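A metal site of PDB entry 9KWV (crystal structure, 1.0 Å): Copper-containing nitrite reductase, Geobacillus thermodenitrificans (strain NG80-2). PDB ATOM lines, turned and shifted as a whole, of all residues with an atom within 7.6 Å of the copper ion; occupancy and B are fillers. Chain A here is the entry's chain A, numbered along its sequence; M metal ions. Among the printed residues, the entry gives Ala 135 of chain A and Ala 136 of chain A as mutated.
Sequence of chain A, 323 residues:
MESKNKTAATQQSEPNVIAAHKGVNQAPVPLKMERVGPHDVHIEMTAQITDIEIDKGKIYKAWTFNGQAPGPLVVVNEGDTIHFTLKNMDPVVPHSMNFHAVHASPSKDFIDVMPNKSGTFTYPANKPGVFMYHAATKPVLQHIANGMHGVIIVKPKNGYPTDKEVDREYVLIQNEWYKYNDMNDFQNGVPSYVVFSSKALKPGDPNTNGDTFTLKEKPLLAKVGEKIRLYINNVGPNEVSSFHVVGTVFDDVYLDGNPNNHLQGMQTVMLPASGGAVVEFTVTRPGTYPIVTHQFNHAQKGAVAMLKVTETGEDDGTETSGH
Trp 63 touches the copper ion (CE3 to CU, 3.95 Å).
Ala 135 touches the copper ion.
Five residues have an atom within 4 Å of the copper ion: Trp 63, His 95, Ala 135, His 143 and Met 148.
O of Val 93 sits close to NE2 of His 95 (3.3 Å).
NE2 of His 95 is in hydrogen-bond range of OD2 of Asp 90 (2.8 Å).
N of Ala 135 lies within hydrogen-bond range of O of Met 148, 3.2 Å away.
N of Met 148 sits close to O of Trp 63 (3.2 Å).
The backbone carbonyl oxygen of Asn 146 lies within hydrogen-bond range of the backbone NH of Trp 63.
The copper ion is bound by a ring nitrogen (ND1) of His 143, a ring nitrogen (ND1) of His 95 and the side-chain sulfur of Met 148.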
ATOM      1  N   ALA A  47      28.244  -1.289 -20.464  1.00  0.00           N
ATOM      2  CA  ALA A  47      27.087  -0.432 -20.710  1.00  0.00           C
ATOM      3  C   ALA A  47      27.075  -0.152 -22.203  1.00  0.00           C
ATOM      4  O   ALA A  47      28.088   0.299 -22.758  1.00  0.00           O
ATOM      5  CB  ALA A  47      27.187   0.874 -19.920  1.00  0.00           C
ATOM      6  N   GLN A  48      25.968  -0.446 -22.871  1.00  0.00           N
ATOM      7  CA  GLN A  48      25.932  -0.344 -24.322  1.00  0.00           C
ATOM      8  C   GLN A  48      24.507  -0.097 -24.803  1.00  0.00           C
ATOM      9  O   GLN A  48      23.530  -0.360 -24.087  1.00  0.00           O
ATOM     10  CB  GLN A  48      26.544  -1.598 -24.971  1.00  0.00           C
ATOM     11  CG  GLN A  48      25.797  -2.887 -24.658  1.00  0.00           C
ATOM     12  CD  GLN A  48      26.468  -4.068 -25.318  1.00  0.00           C
ATOM     13  OE1 GLN A  48      27.440  -4.628 -24.810  1.00  0.00           O
ATOM     14  NE2 GLN A  48      25.992  -4.429 -26.489  1.00  0.00           N
ATOM     15  N   ILE A  49      24.418   0.423 -26.016  1.00  0.00           N
ATOM     16  CA  ILE A  49      23.177   0.872 -26.636  1.00  0.00           C
ATOM     17  C   ILE A  49      22.792  -0.151 -27.692  1.00  0.00           C
ATOM     18  O   ILE A  49      23.532  -0.334 -28.672  1.00  0.00           O
ATOM     19  CB  ILE A  49      23.377   2.267 -27.248  1.00  0.00           C
ATOM     20  CG1 ILE A  49      23.858   3.292 -26.186  1.00  0.00           C
ATOM     21  CG2 ILE A  49      22.106   2.735 -27.953  1.00  0.00           C
ATOM     22  CD1 ILE A  49      22.942   3.410 -24.972  1.00  0.00           C
ATOM     23  N   TRP A  63      19.105   1.327 -23.349  1.00  0.00           N
ATOM     24  CA  TRP A  63      20.311   1.507 -22.558  1.00  0.00           C
ATOM     25  C   TRP A  63      20.474   0.243 -21.737  1.00  0.00           C
ATOM     26  O   TRP A  63      19.614  -0.077 -20.922  1.00  0.00           O
ATOM     27  CB  TRP A  63      20.167   2.710 -21.641  1.00  0.00           C
ATOM     28  CG  TRP A  63      19.961   4.056 -22.298  1.00  0.00           C
ATOM     29  CD1 TRP A  63      19.718   4.328 -23.625  1.00  0.00           C
ATOM     30  CD2 TRP A  63      19.966   5.314 -21.629  1.00  0.00           C
ATOM     31  NE1 TRP A  63      19.591   5.690 -23.800  1.00  0.00           N
ATOM     32  CE2 TRP A  63      19.741   6.311 -22.588  1.00  0.00           C
ATOM     33  CE3 TRP A  63      20.129   5.692 -20.292  1.00  0.00           C
ATOM     34  CZ2 TRP A  63      19.666   7.665 -22.252  1.00  0.00           C
ATOM     35  CZ3 TRP A  63      20.058   7.030 -19.959  1.00  0.00           C
ATOM     36  CH2 TRP A  63      19.839   8.000 -20.931  1.00  0.00           C
ATOM     37  N   THR A  64      21.555  -0.515 -21.979  1.00  0.00           N
ATOM     38  CA  THR A  64      21.651  -1.875 -21.478  1.00  0.00           C
ATOM     39  C   THR A  64      22.982  -2.157 -20.807  1.00  0.00           C
ATOM     40  O   THR A  64      23.998  -1.502 -21.061  1.00  0.00           O
ATOM     41  CB  THR A  64      21.501  -2.933 -22.586  1.00  0.00           C
ATOM     42  OG1 THR A  64      22.692  -3.018 -23.380  1.00  0.00           O
ATOM     43  CG2 THR A  64      20.303  -2.655 -23.480  1.00  0.00           C
ATOM     44  N   PHE A  65      22.951  -3.187 -19.964  1.00  0.00           N
ATOM     45  CA  PHE A  65      24.136  -3.946 -19.610  1.00  0.00           C
ATOM     46  C   PHE A  65      24.274  -5.103 -20.595  1.00  0.00           C
ATOM     47  O   PHE A  65      23.375  -5.945 -20.717  1.00  0.00           O
ATOM     48  CB  PHE A  65      24.043  -4.445 -18.179  1.00  0.00           C
ATOM     49  CG  PHE A  65      23.948  -3.339 -17.145  1.00  0.00           C
ATOM     50  CD1 PHE A  65      25.041  -2.527 -16.886  1.00  0.00           C
ATOM     51  CD2 PHE A  65      22.769  -3.090 -16.473  1.00  0.00           C
ATOM     52  CE1 PHE A  65      24.970  -1.513 -15.946  1.00  0.00           C
ATOM     53  CE2 PHE A  65      22.699  -2.073 -15.516  1.00  0.00           C
ATOM     54  CZ  PHE A  65      23.791  -1.285 -15.264  1.00  0.00           C
ATOM     55  N   LEU A  86      32.804  -2.164 -14.887  1.00  0.00           N
ATOM     56  CA  LEU A  86      31.898  -1.701 -15.922  1.00  0.00           C
ATOM     57  C   LEU A  86      32.705  -1.003 -17.005  1.00  0.00           C
ATOM     58  O   LEU A  86      33.449  -0.056 -16.725  1.00  0.00           O
ATOM     59  CB  LEU A  86      30.859  -0.715 -15.357  1.00  0.00           C
ATOM     60  CG  LEU A  86      29.788  -0.227 -16.347  1.00  0.00           C
ATOM     61  CD1 LEU A  86      28.889  -1.372 -16.821  1.00  0.00           C
ATOM     62  CD2 LEU A  86      28.955   0.867 -15.719  1.00  0.00           C
ATOM     63  N   ASN A  88      32.154   1.203 -20.203  1.00  0.00           N
ATOM     64  CA  ASN A  88      31.101   2.029 -20.802  1.00  0.00           C
ATOM     65  C   ASN A  88      31.375   2.224 -22.287  1.00  0.00           C
ATOM     66  O   ASN A  88      32.287   2.956 -22.669  1.00  0.00           O
ATOM     67  CB  ASN A  88      30.971   3.378 -20.096  1.00  0.00           C
ATOM     68  CG  ASN A  88      29.768   4.153 -20.571  1.00  0.00           C
ATOM     69  OD1 ASN A  88      29.024   3.689 -21.436  1.00  0.00           O
ATOM     70  ND2 ASN A  88      29.567   5.337 -20.018  1.00  0.00           N
ATOM     71  N   ASP A  90      28.932   3.389 -24.330  1.00  0.00           N
ATOM     72  CA  ASP A  90      28.076   4.468 -24.813  1.00  0.00           C
ATOM     73  C   ASP A  90      28.968   5.627 -25.231  1.00  0.00           C
ATOM     74  O   ASP A  90      29.863   6.018 -24.477  1.00  0.00           O
ATOM     75  CB  ASP A  90      27.147   4.879 -23.661  1.00  0.00           C
ATOM     76  CG  ASP A  90      26.046   5.859 -24.070  1.00  0.00           C
ATOM     77  OD1 ASP A  90      26.334   6.801 -24.838  1.00  0.00           O
ATOM     78  OD2 ASP A  90      24.917   5.710 -23.545  1.00  0.00           O
ATOM     79  N   VAL A  93      26.791   9.066 -22.943  1.00  0.00           N
ATOM     80  CA  VAL A  93      26.112   9.065 -21.646  1.00  0.00           C
ATOM     81  C   VAL A  93      26.938   8.291 -20.628  1.00  0.00           C
ATOM     82  O   VAL A  93      27.311   7.135 -20.895  1.00  0.00           O
ATOM     83  CB  VAL A  93      24.677   8.494 -21.735  1.00  0.00           C
ATOM     84  CG1 VAL A  93      23.964   8.671 -20.401  1.00  0.00           C
ATOM     85  CG2 VAL A  93      23.891   9.149 -22.850  1.00  0.00           C
ATOM     86  N   PRO A  94      27.206   8.858 -19.440  1.00  0.00           N
ATOM     87  CA  PRO A  94      27.800   8.063 -18.352  1.00  0.00           C
ATOM     88  C   PRO A  94      26.809   7.019 -17.845  1.00  0.00           C
ATOM     89  O   PRO A  94      25.595   7.223 -17.881  1.00  0.00           O
ATOM     90  CB  PRO A  94      28.085   9.108 -17.266  1.00  0.00           C
ATOM     91  CG  PRO A  94      28.061  10.425 -17.963  1.00  0.00           C
ATOM     92  CD  PRO A  94      27.020  10.260 -19.031  1.00  0.00           C
ATOM     93  N   HIS A  95      27.342   5.917 -17.330  1.00  0.00           N
ATOM     94  CA  HIS A  95      26.534   4.882 -16.687  1.00  0.00           C
ATOM     95  C   HIS A  95      27.250   4.390 -15.435  1.00  0.00           C
ATOM     96  O   HIS A  95      28.371   4.796 -15.138  1.00  0.00           O
ATOM     97  CB  HIS A  95      26.212   3.729 -17.661  1.00  0.00           C
ATOM     98  CG  HIS A  95      25.497   4.171 -18.902  1.00  0.00           C
ATOM     99  ND1 HIS A  95      24.161   4.515 -18.930  1.00  0.00           N
ATOM    100  CD2 HIS A  95      25.963   4.355 -20.159  1.00  0.00           C
ATOM    101  CE1 HIS A  95      23.840   4.884 -20.166  1.00  0.00           C
ATOM    102  NE2 HIS A  95      24.922   4.801 -20.931  1.00  0.00           N
ATOM    103  N   SER A  96      26.591   3.526 -14.663  1.00  0.00           N
ATOM    104  CA  SER A  96      27.084   3.103 -13.361  1.00  0.00           C
ATOM    105  C   SER A  96      26.305   1.856 -12.955  1.00  0.00           C
ATOM    106  O   SER A  96      25.394   1.410 -13.668  1.00  0.00           O
ATOM    107  CB  SER A  96      26.874   4.200 -12.319  1.00  0.00           C
ATOM    108  OG  SER A  96      25.480   4.475 -12.177  1.00  0.00           O
ATOM    109  N   HIS A 134      20.864  -2.232 -11.027  1.00  0.00           N
ATOM    110  CA  HIS A 134      20.446  -1.204 -11.982  1.00  0.00           C
ATOM    111  C   HIS A 134      21.493  -0.091 -11.993  1.00  0.00           C
ATOM    112  O   HIS A 134      22.325   0.020 -11.091  1.00  0.00           O
ATOM    113  CB  HIS A 134      19.062  -0.636 -11.628  1.00  0.00           C
ATOM    114  CG  HIS A 134      18.994  -0.022 -10.267  1.00  0.00           C
ATOM    115  ND1 HIS A 134      19.368   1.285 -10.022  1.00  0.00           N
ATOM    116  CD2 HIS A 134      18.559  -0.508  -9.075  1.00  0.00           C
ATOM    117  CE1 HIS A 134      19.168   1.565  -8.735  1.00  0.00           C
ATOM    118  NE2 HIS A 134      18.659   0.501  -8.149  1.00  0.00           N
ATOM    119  N   ALA A 135      21.408   0.766 -13.008  1.00  0.00           N
ATOM    120  CA  ALA A 135      22.294   1.921 -13.030  1.00  0.00           C
ATOM    121  C   ALA A 135      21.921   2.930 -11.950  1.00  0.00           C
ATOM    122  O   ALA A 135      20.755   3.076 -11.576  1.00  0.00           O
ATOM    123  CB  ALA A 135      22.278   2.582 -14.410  1.00  0.00           C
ATOM    124  N   ALA A 136      22.930   3.661 -11.464  1.00  0.00           N
ATOM    125  CA  ALA A 136      22.784   4.614 -10.367  1.00  0.00           C
ATOM    126  C   ALA A 136      22.945   6.054 -10.809  1.00  0.00           C
ATOM    127  O   ALA A 136      22.930   6.967  -9.970  1.00  0.00           O
ATOM    128  CB  ALA A 136      23.752   4.278  -9.225  1.00  0.00           C
ATOM    129  N   THR A 137      23.018   6.298 -12.099  1.00  0.00           N
ATOM    130  CA  THR A 137      23.332   7.606 -12.653  1.00  0.00           C
ATOM    131  C   THR A 137      22.079   8.462 -12.693  1.00  0.00           C
ATOM    132  O   THR A 137      21.019   8.016 -13.150  1.00  0.00           O
ATOM    133  CB  THR A 137      23.899   7.394 -14.061  1.00  0.00           C
ATOM    134  OG1 THR A 137      25.067   6.554 -14.002  1.00  0.00           O
ATOM    135  CG2 THR A 137      24.248   8.710 -14.747  1.00  0.00           C
ATOM    136  N   PRO A 139      19.384  11.056 -13.994  1.00  0.00           N
ATOM    137  CA  PRO A 139      18.219  10.597 -13.217  1.00  0.00           C
ATOM    138  C   PRO A 139      18.097   9.086 -13.281  1.00  0.00           C
ATOM    139  O   PRO A 139      18.036   8.506 -14.377  1.00  0.00           O
ATOM    140  CB  PRO A 139      17.025  11.253 -13.934  1.00  0.00           C
ATOM    141  CG  PRO A 139      17.581  12.098 -15.009  1.00  0.00           C
ATOM    142  CD  PRO A 139      18.977  11.617 -15.287  1.00  0.00           C
ATOM    143  N   VAL A 140      18.040   8.442 -12.113  1.00  0.00           N
ATOM    144  CA  VAL A 140      17.992   6.994 -12.076  1.00  0.00           C
ATOM    145  C   VAL A 140      16.761   6.470 -12.809  1.00  0.00           C
ATOM    146  O   VAL A 140      16.823   5.449 -13.511  1.00  0.00           O
ATOM    147  CB  VAL A 140      18.095   6.492 -10.626  1.00  0.00           C
ATOM    148  CG1 VAL A 140      17.810   5.016 -10.524  1.00  0.00           C
ATOM    149  CG2 VAL A 140      19.497   6.798 -10.076  1.00  0.00           C
ATOM    150  N   GLN A 142      15.431   7.553 -15.472  1.00  0.00           N
ATOM    151  CA  GLN A 142      15.713   7.511 -16.911  1.00  0.00           C
ATOM    152  C   GLN A 142      16.523   6.270 -17.284  1.00  0.00           C
ATOM    153  O   GLN A 142      16.246   5.602 -18.292  1.00  0.00           O
ATOM    154  CB  GLN A 142      16.464   8.780 -17.315  1.00  0.00           C
ATOM    155  CG  GLN A 142      16.628   8.936 -18.822  1.00  0.00           C
ATOM    156  CD  GLN A 142      17.232  10.257 -19.204  1.00  0.00           C
ATOM    157  OE1 GLN A 142      17.795  10.969 -18.379  1.00  0.00           O
ATOM    158  NE2 GLN A 142      17.122  10.599 -20.475  1.00  0.00           N
ATOM    159  N   HIS A 143      17.550   5.960 -16.480  1.00  0.00           N
ATOM    160  CA  HIS A 143      18.388   4.803 -16.771  1.00  0.00           C
ATOM    161  C   HIS A 143      17.631   3.494 -16.601  1.00  0.00           C
ATOM    162  O   HIS A 143      17.767   2.597 -17.444  1.00  0.00           O
ATOM    163  CB  HIS A 143      19.658   4.819 -15.915  1.00  0.00           C
ATOM    164  CG  HIS A 143      20.632   5.879 -16.330  1.00  0.00           C
ATOM    165  ND1 HIS A 143      21.776   5.605 -17.054  1.00  0.00           N
ATOM    166  CD2 HIS A 143      20.583   7.224 -16.182  1.00  0.00           C
ATOM    167  CE1 HIS A 143      22.396   6.744 -17.301  1.00  0.00           C
ATOM    168  NE2 HIS A 143      21.691   7.740 -16.785  1.00  0.00           N
ATOM    169  N   ILE A 144      16.841   3.361 -15.526  1.00  0.00           N
ATOM    170  CA  ILE A 144      16.066   2.138 -15.354  1.00  0.00           C
ATOM    171  C   ILE A 144      15.044   1.988 -16.473  1.00  0.00           C
ATOM    172  O   ILE A 144      14.934   0.945 -17.115  1.00  0.00           O
ATOM    173  CB  ILE A 144      15.394   2.074 -13.962  1.00  0.00           C
ATOM    174  CG1 ILE A 144      16.441   2.095 -12.830  1.00  0.00           C
ATOM    175  CG2 ILE A 144      14.540   0.817 -13.862  1.00  0.00           C
ATOM    176  CD1 ILE A 144      15.829   2.128 -11.443  1.00  0.00           C
ATOM    177  N   ASN A 146      14.950   3.119 -19.428  1.00  0.00           N
ATOM    178  CA  ASN A 146      15.543   2.835 -20.729  1.00  0.00           C
ATOM    179  C   ASN A 146      16.174   1.448 -20.828  1.00  0.00           C
ATOM    180  O   ASN A 146      16.603   1.066 -21.929  1.00  0.00           O
ATOM    181  CB  ASN A 146      16.570   3.904 -21.113  1.00  0.00           C
ATOM    182  CG  ASN A 146      15.931   5.184 -21.635  1.00  0.00           C
ATOM    183  OD1 ASN A 146      14.871   5.179 -22.250  1.00  0.00           O
ATOM    184  ND2 ASN A 146      16.618   6.303 -21.416  1.00  0.00           N
ATOM    185  N   GLY A 147      16.223   0.666 -19.743  1.00  0.00           N
ATOM    186  CA  GLY A 147      16.630  -0.729 -19.806  1.00  0.00           C
ATOM    187  C   GLY A 147      17.716  -1.173 -18.837  1.00  0.00           C
ATOM    188  O   GLY A 147      18.053  -2.365 -18.853  1.00  0.00           O
ATOM    189  N   MET A 148      18.272  -0.288 -18.004  1.00  0.00           N
ATOM    190  CA  MET A 148      19.456  -0.627 -17.203  1.00  0.00           C
ATOM    191  C   MET A 148      19.012  -1.174 -15.851  1.00  0.00           C
ATOM    192  O   MET A 148      19.109  -0.528 -14.793  1.00  0.00           O
ATOM    193  CB  MET A 148      20.344   0.605 -17.070  1.00  0.00           C
ATOM    194  CG  MET A 148      21.138   0.902 -18.278  1.00  0.00           C
ATOM    195  SD  MET A 148      22.693   1.789 -17.929  1.00  0.00           S
ATOM    196  CE  MET A 148      23.544   1.301 -19.391  1.00  0.00           C
HETATM  197 CU    CU M   1      22.563   3.929 -17.722  1.00  0.00          CU
